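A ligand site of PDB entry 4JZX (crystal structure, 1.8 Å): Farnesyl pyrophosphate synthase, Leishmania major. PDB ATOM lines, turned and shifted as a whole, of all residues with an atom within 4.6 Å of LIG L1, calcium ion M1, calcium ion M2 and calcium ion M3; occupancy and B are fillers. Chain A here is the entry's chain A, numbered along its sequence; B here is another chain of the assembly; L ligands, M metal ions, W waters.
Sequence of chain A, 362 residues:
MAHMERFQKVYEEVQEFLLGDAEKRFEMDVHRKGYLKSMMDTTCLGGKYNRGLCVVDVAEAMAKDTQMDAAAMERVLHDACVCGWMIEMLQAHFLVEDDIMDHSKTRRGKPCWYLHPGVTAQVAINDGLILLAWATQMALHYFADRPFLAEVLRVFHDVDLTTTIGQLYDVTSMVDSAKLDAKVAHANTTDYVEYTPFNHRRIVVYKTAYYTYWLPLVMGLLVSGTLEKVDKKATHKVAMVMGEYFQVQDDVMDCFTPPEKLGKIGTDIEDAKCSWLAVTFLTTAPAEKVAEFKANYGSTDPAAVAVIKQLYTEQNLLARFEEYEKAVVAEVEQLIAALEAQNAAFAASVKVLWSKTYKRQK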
ATOM      1  N   PHE A  94     -21.164  -9.969  27.250  1.00  0.00           N
ATOM      2  CA  PHE A  94     -20.113  -8.954  27.111  1.00  0.00           C
ATOM      3  C   PHE A  94     -18.808  -9.383  27.753  1.00  0.00           C
ATOM      4  O   PHE A  94     -17.747  -9.226  27.156  1.00  0.00           O
ATOM      5  CB  PHE A  94     -20.543  -7.599  27.698  1.00  0.00           C
ATOM      6  CG  PHE A  94     -21.634  -6.894  26.919  1.00  0.00           C
ATOM      7  CD1 PHE A  94     -22.547  -6.062  27.574  1.00  0.00           C
ATOM      8  CD2 PHE A  94     -21.742  -7.036  25.535  1.00  0.00           C
ATOM      9  CE1 PHE A  94     -23.559  -5.406  26.873  1.00  0.00           C
ATOM     10  CE2 PHE A  94     -22.752  -6.375  24.826  1.00  0.00           C
ATOM     11  CZ  PHE A  94     -23.652  -5.567  25.493  1.00  0.00           C
ATOM     12  N   LEU A  95     -18.878  -9.948  28.961  1.00  0.00           N
ATOM     13  CA  LEU A  95     -17.669 -10.313  29.696  1.00  0.00           C
ATOM     14  C   LEU A  95     -16.945 -11.516  29.089  1.00  0.00           C
ATOM     15  O   LEU A  95     -15.709 -11.522  29.040  1.00  0.00           O
ATOM     16  CB  LEU A  95     -17.944 -10.526  31.185  1.00  0.00           C
ATOM     17  CG  LEU A  95     -18.592  -9.377  31.974  1.00  0.00           C
ATOM     18  CD1 LEU A  95     -18.618  -9.704  33.475  1.00  0.00           C
ATOM     19  CD2 LEU A  95     -17.906  -8.045  31.711  1.00  0.00           C
ATOM     20  N   ASP A  98     -15.310  -9.987  25.972  1.00  0.00           N
ATOM     21  CA  ASP A  98     -14.265  -9.044  26.356  1.00  0.00           C
ATOM     22  C   ASP A  98     -13.043  -9.733  26.980  1.00  0.00           C
ATOM     23  O   ASP A  98     -11.905  -9.326  26.738  1.00  0.00           O
ATOM     24  CB  ASP A  98     -14.806  -7.991  27.320  1.00  0.00           C
ATOM     25  CG  ASP A  98     -13.756  -6.958  27.677  1.00  0.00           C
ATOM     26  OD1 ASP A  98     -13.316  -6.217  26.774  1.00  0.00           O
ATOM     27  OD2 ASP A  98     -13.342  -6.923  28.851  1.00  0.00           O
ATOM     28  N   ASP A  99     -13.277 -10.777  27.772  1.00  0.00           N
ATOM     29  CA  ASP A  99     -12.174 -11.516  28.392  1.00  0.00           C
ATOM     30  C   ASP A  99     -11.303 -12.184  27.319  1.00  0.00           C
ATOM     31  O   ASP A  99     -10.084 -12.281  27.473  1.00  0.00           O
ATOM     32  CB  ASP A  99     -12.692 -12.524  29.437  1.00  0.00           C
ATOM     33  CG  ASP A  99     -13.066 -11.853  30.781  1.00  0.00           C
ATOM     34  OD1 ASP A  99     -12.627 -10.705  31.035  1.00  0.00           O
ATOM     35  OD2 ASP A  99     -13.787 -12.489  31.588  1.00  0.00           O
ATOM     36  N   ASP A 102      -9.473  -9.049  25.565  1.00  0.00           N
ATOM     37  CA  ASP A 102      -8.414  -8.511  26.429  1.00  0.00           C
ATOM     38  C   ASP A 102      -7.348  -9.536  26.809  1.00  0.00           C
ATOM     39  O   ASP A 102      -6.347  -9.175  27.424  1.00  0.00           O
ATOM     40  CB  ASP A 102      -9.007  -7.920  27.707  1.00  0.00           C
ATOM     41  CG  ASP A 102      -9.745  -6.615  27.474  1.00  0.00           C
ATOM     42  OD1 ASP A 102      -9.676  -6.051  26.361  1.00  0.00           O
ATOM     43  OD2 ASP A 102     -10.401  -6.144  28.419  1.00  0.00           O
ATOM     44  N   SER A 104      -7.610 -11.895  29.072  1.00  0.00           N
ATOM     45  CA  SER A 104      -7.570 -11.775  30.537  1.00  0.00           C
ATOM     46  C   SER A 104      -7.489 -13.140  31.216  1.00  0.00           C
ATOM     47  O   SER A 104      -7.707 -14.181  30.593  1.00  0.00           O
ATOM     48  CB  SER A 104      -8.791 -11.003  31.040  1.00  0.00           C
ATOM     49  OG  SER A 104      -8.732  -9.648  30.616  1.00  0.00           O
ATOM     50  N   ARG A 107     -11.968 -13.772  36.175  1.00  0.00           N
ATOM     51  CA  ARG A 107     -13.247 -13.080  36.206  1.00  0.00           C
ATOM     52  C   ARG A 107     -14.044 -13.566  37.397  1.00  0.00           C
ATOM     53  O   ARG A 107     -14.232 -14.767  37.547  1.00  0.00           O
ATOM     54  CB  ARG A 107     -14.042 -13.363  34.917  1.00  0.00           C
ATOM     55  CG  ARG A 107     -15.467 -12.780  34.914  1.00  0.00           C
ATOM     56  CD  ARG A 107     -15.447 -11.255  34.941  1.00  0.00           C
ATOM     57  NE  ARG A 107     -14.931 -10.661  33.704  1.00  0.00           N
ATOM     58  CZ  ARG A 107     -14.816  -9.354  33.498  1.00  0.00           C
ATOM     59  NH1 ARG A 107     -15.183  -8.493  34.437  1.00  0.00           N
ATOM     60  NH2 ARG A 107     -14.327  -8.891  32.342  1.00  0.00           N
ATOM     61  N   THR A 163     -23.382  -0.523  23.176  1.00  0.00           N
ATOM     62  CA  THR A 163     -22.228  -1.119  23.856  1.00  0.00           C
ATOM     63  C   THR A 163     -21.155  -1.586  22.859  1.00  0.00           C
ATOM     64  O   THR A 163     -19.956  -1.386  23.094  1.00  0.00           O
ATOM     65  CB  THR A 163     -22.670  -2.267  24.783  1.00  0.00           C
ATOM     66  OG1 THR A 163     -23.772  -1.834  25.601  1.00  0.00           O
ATOM     67  CG2 THR A 163     -21.535  -2.699  25.689  1.00  0.00           C
ATOM     68  N   THR A 164     -21.580  -2.205  21.756  1.00  0.00           N
ATOM     69  CA  THR A 164     -20.617  -2.661  20.733  1.00  0.00           C
ATOM     70  C   THR A 164     -19.860  -1.492  20.090  1.00  0.00           C
ATOM     71  O   THR A 164     -18.684  -1.611  19.772  1.00  0.00           O
ATOM     72  CB  THR A 164     -21.226  -3.597  19.629  1.00  0.00           C
ATOM     73  OG1 THR A 164     -22.106  -2.850  18.772  1.00  0.00           O
ATOM     74  CG2 THR A 164     -21.941  -4.803  20.235  1.00  0.00           C
ATOM     75  N   GLN A 167     -17.408  -0.421  22.656  1.00  0.00           N
ATOM     76  CA  GLN A 167     -16.294  -1.365  22.573  1.00  0.00           C
ATOM     77  C   GLN A 167     -15.375  -1.068  21.395  1.00  0.00           C
ATOM     78  O   GLN A 167     -14.143  -1.157  21.532  1.00  0.00           O
ATOM     79  CB  GLN A 167     -16.798  -2.806  22.495  1.00  0.00           C
ATOM     80  CG  GLN A 167     -15.693  -3.849  22.529  1.00  0.00           C
ATOM     81  CD  GLN A 167     -15.136  -4.103  23.933  1.00  0.00           C
ATOM     82  OE1 GLN A 167     -15.411  -3.357  24.878  1.00  0.00           O
ATOM     83  NE2 GLN A 167     -14.339  -5.167  24.074  1.00  0.00           N
ATOM     84  N   ASP A 170     -13.188   1.637  22.464  1.00  0.00           N
ATOM     85  CA  ASP A 170     -12.233   1.123  23.441  1.00  0.00           C
ATOM     86  C   ASP A 170     -11.065   0.379  22.768  1.00  0.00           C
ATOM     87  O   ASP A 170      -9.896   0.661  23.059  1.00  0.00           O
ATOM     88  CB  ASP A 170     -12.943   0.205  24.447  1.00  0.00           C
ATOM     89  CG  ASP A 170     -11.985  -0.372  25.481  1.00  0.00           C
ATOM     90  OD1 ASP A 170     -12.050   0.063  26.643  1.00  0.00           O
ATOM     91  OD2 ASP A 170     -11.166  -1.230  25.112  1.00  0.00           O
ATOM     92  N   LYS A 207     -19.694   2.303  26.156  1.00  0.00           N
ATOM     93  CA  LYS A 207     -19.368   0.911  26.510  1.00  0.00           C
ATOM     94  C   LYS A 207     -19.980   0.456  27.837  1.00  0.00           C
ATOM     95  O   LYS A 207     -20.148  -0.740  28.065  1.00  0.00           O
ATOM     96  CB  LYS A 207     -17.846   0.631  26.478  1.00  0.00           C
ATOM     97  CG  LYS A 207     -17.094   0.911  27.791  1.00  0.00           C
ATOM     98  CD  LYS A 207     -15.711   0.253  27.813  1.00  0.00           C
ATOM     99  CE  LYS A 207     -14.945   0.691  29.047  1.00  0.00           C
ATOM    100  NZ  LYS A 207     -13.543   0.176  29.088  1.00  0.00           N
ATOM    101  N   THR A 208     -20.341   1.412  28.705  1.00  0.00           N
ATOM    102  CA  THR A 208     -20.758   1.060  30.072  1.00  0.00           C
ATOM    103  C   THR A 208     -22.073   1.679  30.548  1.00  0.00           C
ATOM    104  O   THR A 208     -22.949   0.964  31.055  1.00  0.00           O
ATOM    105  CB  THR A 208     -19.621   1.364  31.092  1.00  0.00           C
ATOM    106  OG1 THR A 208     -18.533   0.470  30.869  1.00  0.00           O
ATOM    107  CG2 THR A 208     -20.115   1.219  32.570  1.00  0.00           C
ATOM    108  N   TYR A 211     -25.734   0.246  29.197  1.00  0.00           N
ATOM    109  CA  TYR A 211     -26.208  -1.068  29.640  1.00  0.00           C
ATOM    110  C   TYR A 211     -26.184  -1.256  31.151  1.00  0.00           C
ATOM    111  O   TYR A 211     -26.911  -2.105  31.687  1.00  0.00           O
ATOM    112  CB  TYR A 211     -25.486  -2.207  28.917  1.00  0.00           C
ATOM    113  CG  TYR A 211     -24.239  -2.770  29.563  1.00  0.00           C
ATOM    114  CD1 TYR A 211     -24.284  -3.956  30.304  1.00  0.00           C
ATOM    115  CD2 TYR A 211     -23.000  -2.154  29.371  1.00  0.00           C
ATOM    116  CE1 TYR A 211     -23.133  -4.493  30.877  1.00  0.00           C
ATOM    117  CE2 TYR A 211     -21.838  -2.688  29.935  1.00  0.00           C
ATOM    118  CZ  TYR A 211     -21.907  -3.850  30.687  1.00  0.00           C
ATOM    119  OH  TYR A 211     -20.749  -4.361  31.217  1.00  0.00           O
ATOM    120  N   GLN A 247     -17.651   3.659  35.553  1.00  0.00           N
ATOM    121  CA  GLN A 247     -16.490   3.215  34.764  1.00  0.00           C
ATOM    122  C   GLN A 247     -15.177   3.860  35.207  1.00  0.00           C
ATOM    123  O   GLN A 247     -14.121   3.223  35.169  1.00  0.00           O
ATOM    124  CB  GLN A 247     -16.709   3.448  33.267  1.00  0.00           C
ATOM    125  CG  GLN A 247     -15.666   2.736  32.413  1.00  0.00           C
ATOM    126  CD  GLN A 247     -15.574   1.248  32.712  1.00  0.00           C
ATOM    127  OE1 GLN A 247     -16.577   0.539  32.702  1.00  0.00           O
ATOM    128  NE2 GLN A 247     -14.362   0.767  32.987  1.00  0.00           N
ATOM    129  N   ASP A 250     -14.092   1.833  38.060  1.00  0.00           N
ATOM    130  CA  ASP A 250     -13.530   0.613  37.508  1.00  0.00           C
ATOM    131  C   ASP A 250     -12.102   0.824  37.011  1.00  0.00           C
ATOM    132  O   ASP A 250     -11.213   0.014  37.287  1.00  0.00           O
ATOM    133  CB  ASP A 250     -14.436   0.057  36.401  1.00  0.00           C
ATOM    134  CG  ASP A 250     -13.996  -1.298  35.922  1.00  0.00           C
ATOM    135  OD1 ASP A 250     -14.214  -2.286  36.657  1.00  0.00           O
ATOM    136  OD2 ASP A 250     -13.426  -1.382  34.816  1.00  0.00           O
ATOM    137  N   LYS A 264     -10.743  -9.831  39.567  1.00  0.00           N
ATOM    138  CA  LYS A 264     -10.204  -9.851  38.210  1.00  0.00           C
ATOM    139  C   LYS A 264      -8.831  -9.197  38.184  1.00  0.00           C
ATOM    140  O   LYS A 264      -8.503  -8.417  39.083  1.00  0.00           O
ATOM    141  CB  LYS A 264     -11.156  -9.145  37.220  1.00  0.00           C
ATOM    142  CG  LYS A 264     -11.357  -7.653  37.483  1.00  0.00           C
ATOM    143  CD  LYS A 264     -12.573  -7.095  36.757  1.00  0.00           C
ATOM    144  CE  LYS A 264     -12.731  -5.600  37.053  1.00  0.00           C
ATOM    145  NZ  LYS A 264     -14.005  -5.056  36.486  1.00  0.00           N
ATOM    146  N   ASP A 268      -4.834  -2.683  32.141  1.00  0.00           N
ATOM    147  CA  ASP A 268      -4.980  -1.398  31.461  1.00  0.00           C
ATOM    148  C   ASP A 268      -3.630  -0.765  31.122  1.00  0.00           C
ATOM    149  O   ASP A 268      -3.426  -0.236  30.024  1.00  0.00           O
ATOM    150  CB  ASP A 268      -5.813  -0.425  32.298  1.00  0.00           C
ATOM    151  CG  ASP A 268      -7.303  -0.727  32.268  1.00  0.00           C
ATOM    152  OD1 ASP A 268      -7.734  -1.680  31.564  1.00  0.00           O
ATOM    153  OD2 ASP A 268      -8.049   0.002  32.951  1.00  0.00           O
ATOM    154  N   ASN B 126     -15.559  -8.174  18.078  1.00  0.00           N
ATOM    155  CA  ASN B 126     -16.498  -7.084  18.257  1.00  0.00           C
ATOM    156  C   ASN B 126     -17.117  -6.571  16.952  1.00  0.00           C
ATOM    157  O   ASN B 126     -18.296  -6.222  16.922  1.00  0.00           O
ATOM    158  CB  ASN B 126     -15.876  -5.933  19.045  1.00  0.00           C
ATOM    159  CG  ASN B 126     -16.914  -4.926  19.487  1.00  0.00           C
ATOM    160  OD1 ASN B 126     -17.806  -5.251  20.286  1.00  0.00           O
ATOM    161  ND2 ASN B 126     -16.821  -3.711  18.962  1.00  0.00           N
ATOM    162  N   LEU B 129     -20.049  -8.483  16.320  1.00  0.00           N
ATOM    163  CA  LEU B 129     -21.151  -8.123  17.211  1.00  0.00           C
ATOM    164  C   LEU B 129     -21.895  -6.887  16.674  1.00  0.00           C
ATOM    165  O   LEU B 129     -23.117  -6.831  16.732  1.00  0.00           O
ATOM    166  CB  LEU B 129     -20.666  -7.897  18.644  1.00  0.00           C
ATOM    167  CG  LEU B 129     -19.966  -9.063  19.357  1.00  0.00           C
ATOM    168  CD1 LEU B 129     -19.592  -8.644  20.767  1.00  0.00           C
ATOM    169  CD2 LEU B 129     -20.841 -10.305  19.355  1.00  0.00           C
HETATM  170  O1  LIG L   1     -14.662  -5.822  33.759  1.00  0.00           O
HETATM  171  P1  LIG L   1     -13.493  -5.329  32.924  1.00  0.00           P
HETATM  172  O2  LIG L   1     -12.880  -6.420  32.080  1.00  0.00           O
HETATM  173  O3  LIG L   1     -12.496  -4.538  33.728  1.00  0.00           O
HETATM  174  C1  LIG L   1     -14.282  -4.167  31.731  1.00  0.00           C
HETATM  175  P2  LIG L   1     -13.132  -3.241  30.657  1.00  0.00           P
HETATM  176  O4  LIG L   1     -12.251  -4.227  29.914  1.00  0.00           O
HETATM  177  O5  LIG L   1     -13.985  -2.403  29.741  1.00  0.00           O
HETATM  178  O6  LIG L   1     -12.337  -2.351  31.602  1.00  0.00           O
HETATM  179  C2  LIG L   1     -15.277  -5.024  30.934  1.00  0.00           C
HETATM  180  N1  LIG L   1     -16.214  -4.332  30.034  1.00  0.00           N
HETATM  181  C3  LIG L   1     -16.475  -4.964  28.881  1.00  0.00           C
HETATM  182  C4  LIG L   1     -17.335  -4.442  27.927  1.00  0.00           C
HETATM  183  C5  LIG L   1     -17.969  -3.229  28.201  1.00  0.00           C
HETATM  184  C6  LIG L   1     -17.702  -2.577  29.414  1.00  0.00           C
HETATM  185  C7  LIG L   1     -16.818  -3.159  30.337  1.00  0.00           C
HETATM  186  C8  LIG L   1     -17.506  -5.270  26.660  1.00  0.00           C
HETATM  187  C9  LIG L   1     -18.587  -4.832  25.685  1.00  0.00           C
HETATM  188  C10 LIG L   1     -18.497  -5.694  24.434  1.00  0.00           C
HETATM  189  C11 LIG L   1     -19.464  -5.223  23.359  1.00  0.00           C
HETATM  190  C1  LG2 L   2     -17.891  -5.285  34.911  1.00  0.00           C
HETATM  191  O1  LG2 L   2     -19.102  -4.877  35.551  1.00  0.00           O
HETATM  192  C2  LG2 L   2     -17.741  -4.557  33.569  1.00  0.00           C
HETATM  193  C3  LG2 L   2     -17.792  -3.055  33.735  1.00  0.00           C
HETATM  194  C4  LG2 L   2     -16.916  -2.398  34.495  1.00  0.00           C
HETATM  195  C5  LG2 L   2     -18.878  -2.294  33.037  1.00  0.00           C
HETATM  196  P1  LG2 L   2     -19.412  -5.211  37.090  1.00  0.00           P
HETATM  197  O2  LG2 L   2     -20.813  -4.752  37.359  1.00  0.00           O
HETATM  198  O3  LG2 L   2     -18.303  -4.647  37.967  1.00  0.00           O
HETATM  199  O4  LG2 L   2     -19.303  -6.828  37.149  1.00  0.00           O
HETATM  200  P2  LG2 L   2     -20.223  -7.945  37.913  1.00  0.00           P
HETATM  201  O5  LG2 L   2     -20.727  -7.368  39.211  1.00  0.00           O
HETATM  202  O6  LG2 L   2     -21.316  -8.278  36.919  1.00  0.00           O
HETATM  203  O7  LG2 L   2     -19.200  -9.054  38.045  1.00  0.00           O
HETATM  204 CA    CA M   1     -11.939  -4.466  27.508  1.00  0.00          CA
HETATM  205 CA    CA M   2     -11.635  -2.401  33.736  1.00  0.00          CA
HETATM  206 CA    CA M   3     -11.609  -6.441  30.337  1.00  0.00          CA
HETATM  207  O   HOH W   1     -10.800  -2.434  27.764  1.00  0.00           O
HETATM  208  O   HOH W   2     -11.598  -3.906  25.200  1.00  0.00           O
HETATM  209  O   HOH W   3      -9.727  -5.958  31.591  1.00  0.00           O
HETATM  210  O   HOH W   4     -13.839  -3.121  27.144  1.00  0.00           O
HETATM  211  O   HOH W   5     -10.997  -2.587  36.107  1.00  0.00           O
HETATM  212  O   HOH W   6     -10.185  -1.278  30.233  1.00  0.00           O
HETATM  213  O   HOH W   7      -9.415  -3.200  33.282  1.00  0.00           O
HETATM  214  O   HOH W   8     -11.118  -8.687  30.464  1.00  0.00           O
HETATM  215  O   HOH W   9     -10.652  -0.246  33.387  1.00  0.00           O
HETATM  216  O   HOH W  10     -10.153  -5.882  34.575  1.00  0.00           O
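The side-chain amino group (NZ) of Lys 207 lies within salt-bridge range of an oxygen (O5) of LIG L1. O1 of LIG L1 lies within salt-bridge range of NH1 of Arg 107 (2.8 Å). O1 of LIG L1 lies within salt-bridge range of NZ of Lys 264, at 2.9 Å.
The side-chain amino group of Lys 264 lies within salt-bridge range of the side-chain carboxylate of Asp 250, at 2.8 Å. OD2 of Asp 250 sits close to NE2 of Gln 247 (3.0 Å). OD1 of Asp 98 sits close to NE2 of Gln 167 (3.1 Å). The side-chain amino group of Lys 207 lies within salt-bridge range of the side-chain carboxylate of Asp 170. NH2 of Arg 107 lies within salt-bridge range of OD1 of Asp 99. OG1 of Thr 208 is in hydrogen-bond range of OE1 of Gln 247. The side-chain amide nitrogen (ND2) of Asn 126 of chain B sits at hydrogen-bond distance from the backbone carbonyl oxygen (O) of Thr 164 (2.9 Å).
Phe 94 touches LIG L1. Thr 163 touches LIG L1. CA of Thr 164 touches C11 of LIG L1, at 3.8 Å. OE1 of Gln 167 touches C8 of LIG L1, 3.4 Å away. Thr 208 touches LIG L1 (OG1 to C6, 3.5 Å). Tyr 211 touches LIG L1. Gln 247 touches LIG L1 (NE2 to O6, 3.97 Å). Asn 126 of chain B touches LIG L1. Hydrophobic or aromatic side chains within 4 Å of LIG L1: Phe 94. The nearest printed residue that does not touch LIG L1 is Leu 95 (4.1 Å).
Within 4 Å of calcium ion M1: Asp 98 and Asp 102.
One residue has an atom within 4 Å of calcium ion M2: Asp 250.
Of the 20 residues printed, 2 come within 4 Å of calcium ion M3. Along chain A the residues within 4 Å of calcium ion M3 span positions 98 to 102. The nearest printed residue that does not touch calcium ion M3 is Arg 107 (4.2 Å).
Water W1 is bound to calcium ion M1, at 2.3 Å. Calcium ion M1 is bound by OD1 of Asp 98. Water W4 is bound to calcium ion M1 (2.4 Å). Water W2 binds calcium ion M1 (2.4 Å). An oxygen (O4) of LIG L1 is bound to calcium ion M1, at 2.4 Å. The side-chain carboxylate (OD2) of Asp 102 is bound to calcium ion M1, 2.5 Å away. Calcium ion M1 has six donor atoms within binding distance. Slightly farther from calcium ion M1 lies the side-chain carboxylate (OD1) of Asp 102 (3.0 Å). Slightly farther from calcium ion M1 lies OD2 of Asp 98 (3.1 Å).
Calcium ion M2 is bound by an oxygen (O6) of LIG L1 (2.2 Å), an oxygen (O3) of LIG L1 (2.3 Å), the side-chain carboxylate of Asp 250 (2.3 Å), water W9 (2.4 Å), water W7 (2.4 Å) and water W5 (2.5 Å).
Calcium ion M3 is bound by an oxygen (O2) of LIG L1 (2.2 Å), the side-chain carboxylate (OD2) of Asp 102 (2.3 Å), water W8 (2.3 Å), water W3 (2.3 Å), the side-chain carboxylate (OD2) of Asp 98 (2.3 Å) and an oxygen (O4) of LIG L1 (2.3 Å).
Water W4 lies within hydrogen-bond range of an oxygen (O5) of LIG L1 (2.7 Å) and the side-chain amide oxygen (OE1) of Gln 167 (2.8 Å). Water W2 lies within hydrogen-bond range of OD2 of Asp 170, OD1 of Asp 102 and NE2 of Gln 167. Water W8 bridges the side-chain hydroxyl (OG) of Ser 104 (2.6 Å) and the side-chain carboxylate (OD1) of Asp 99 (2.6 Å).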
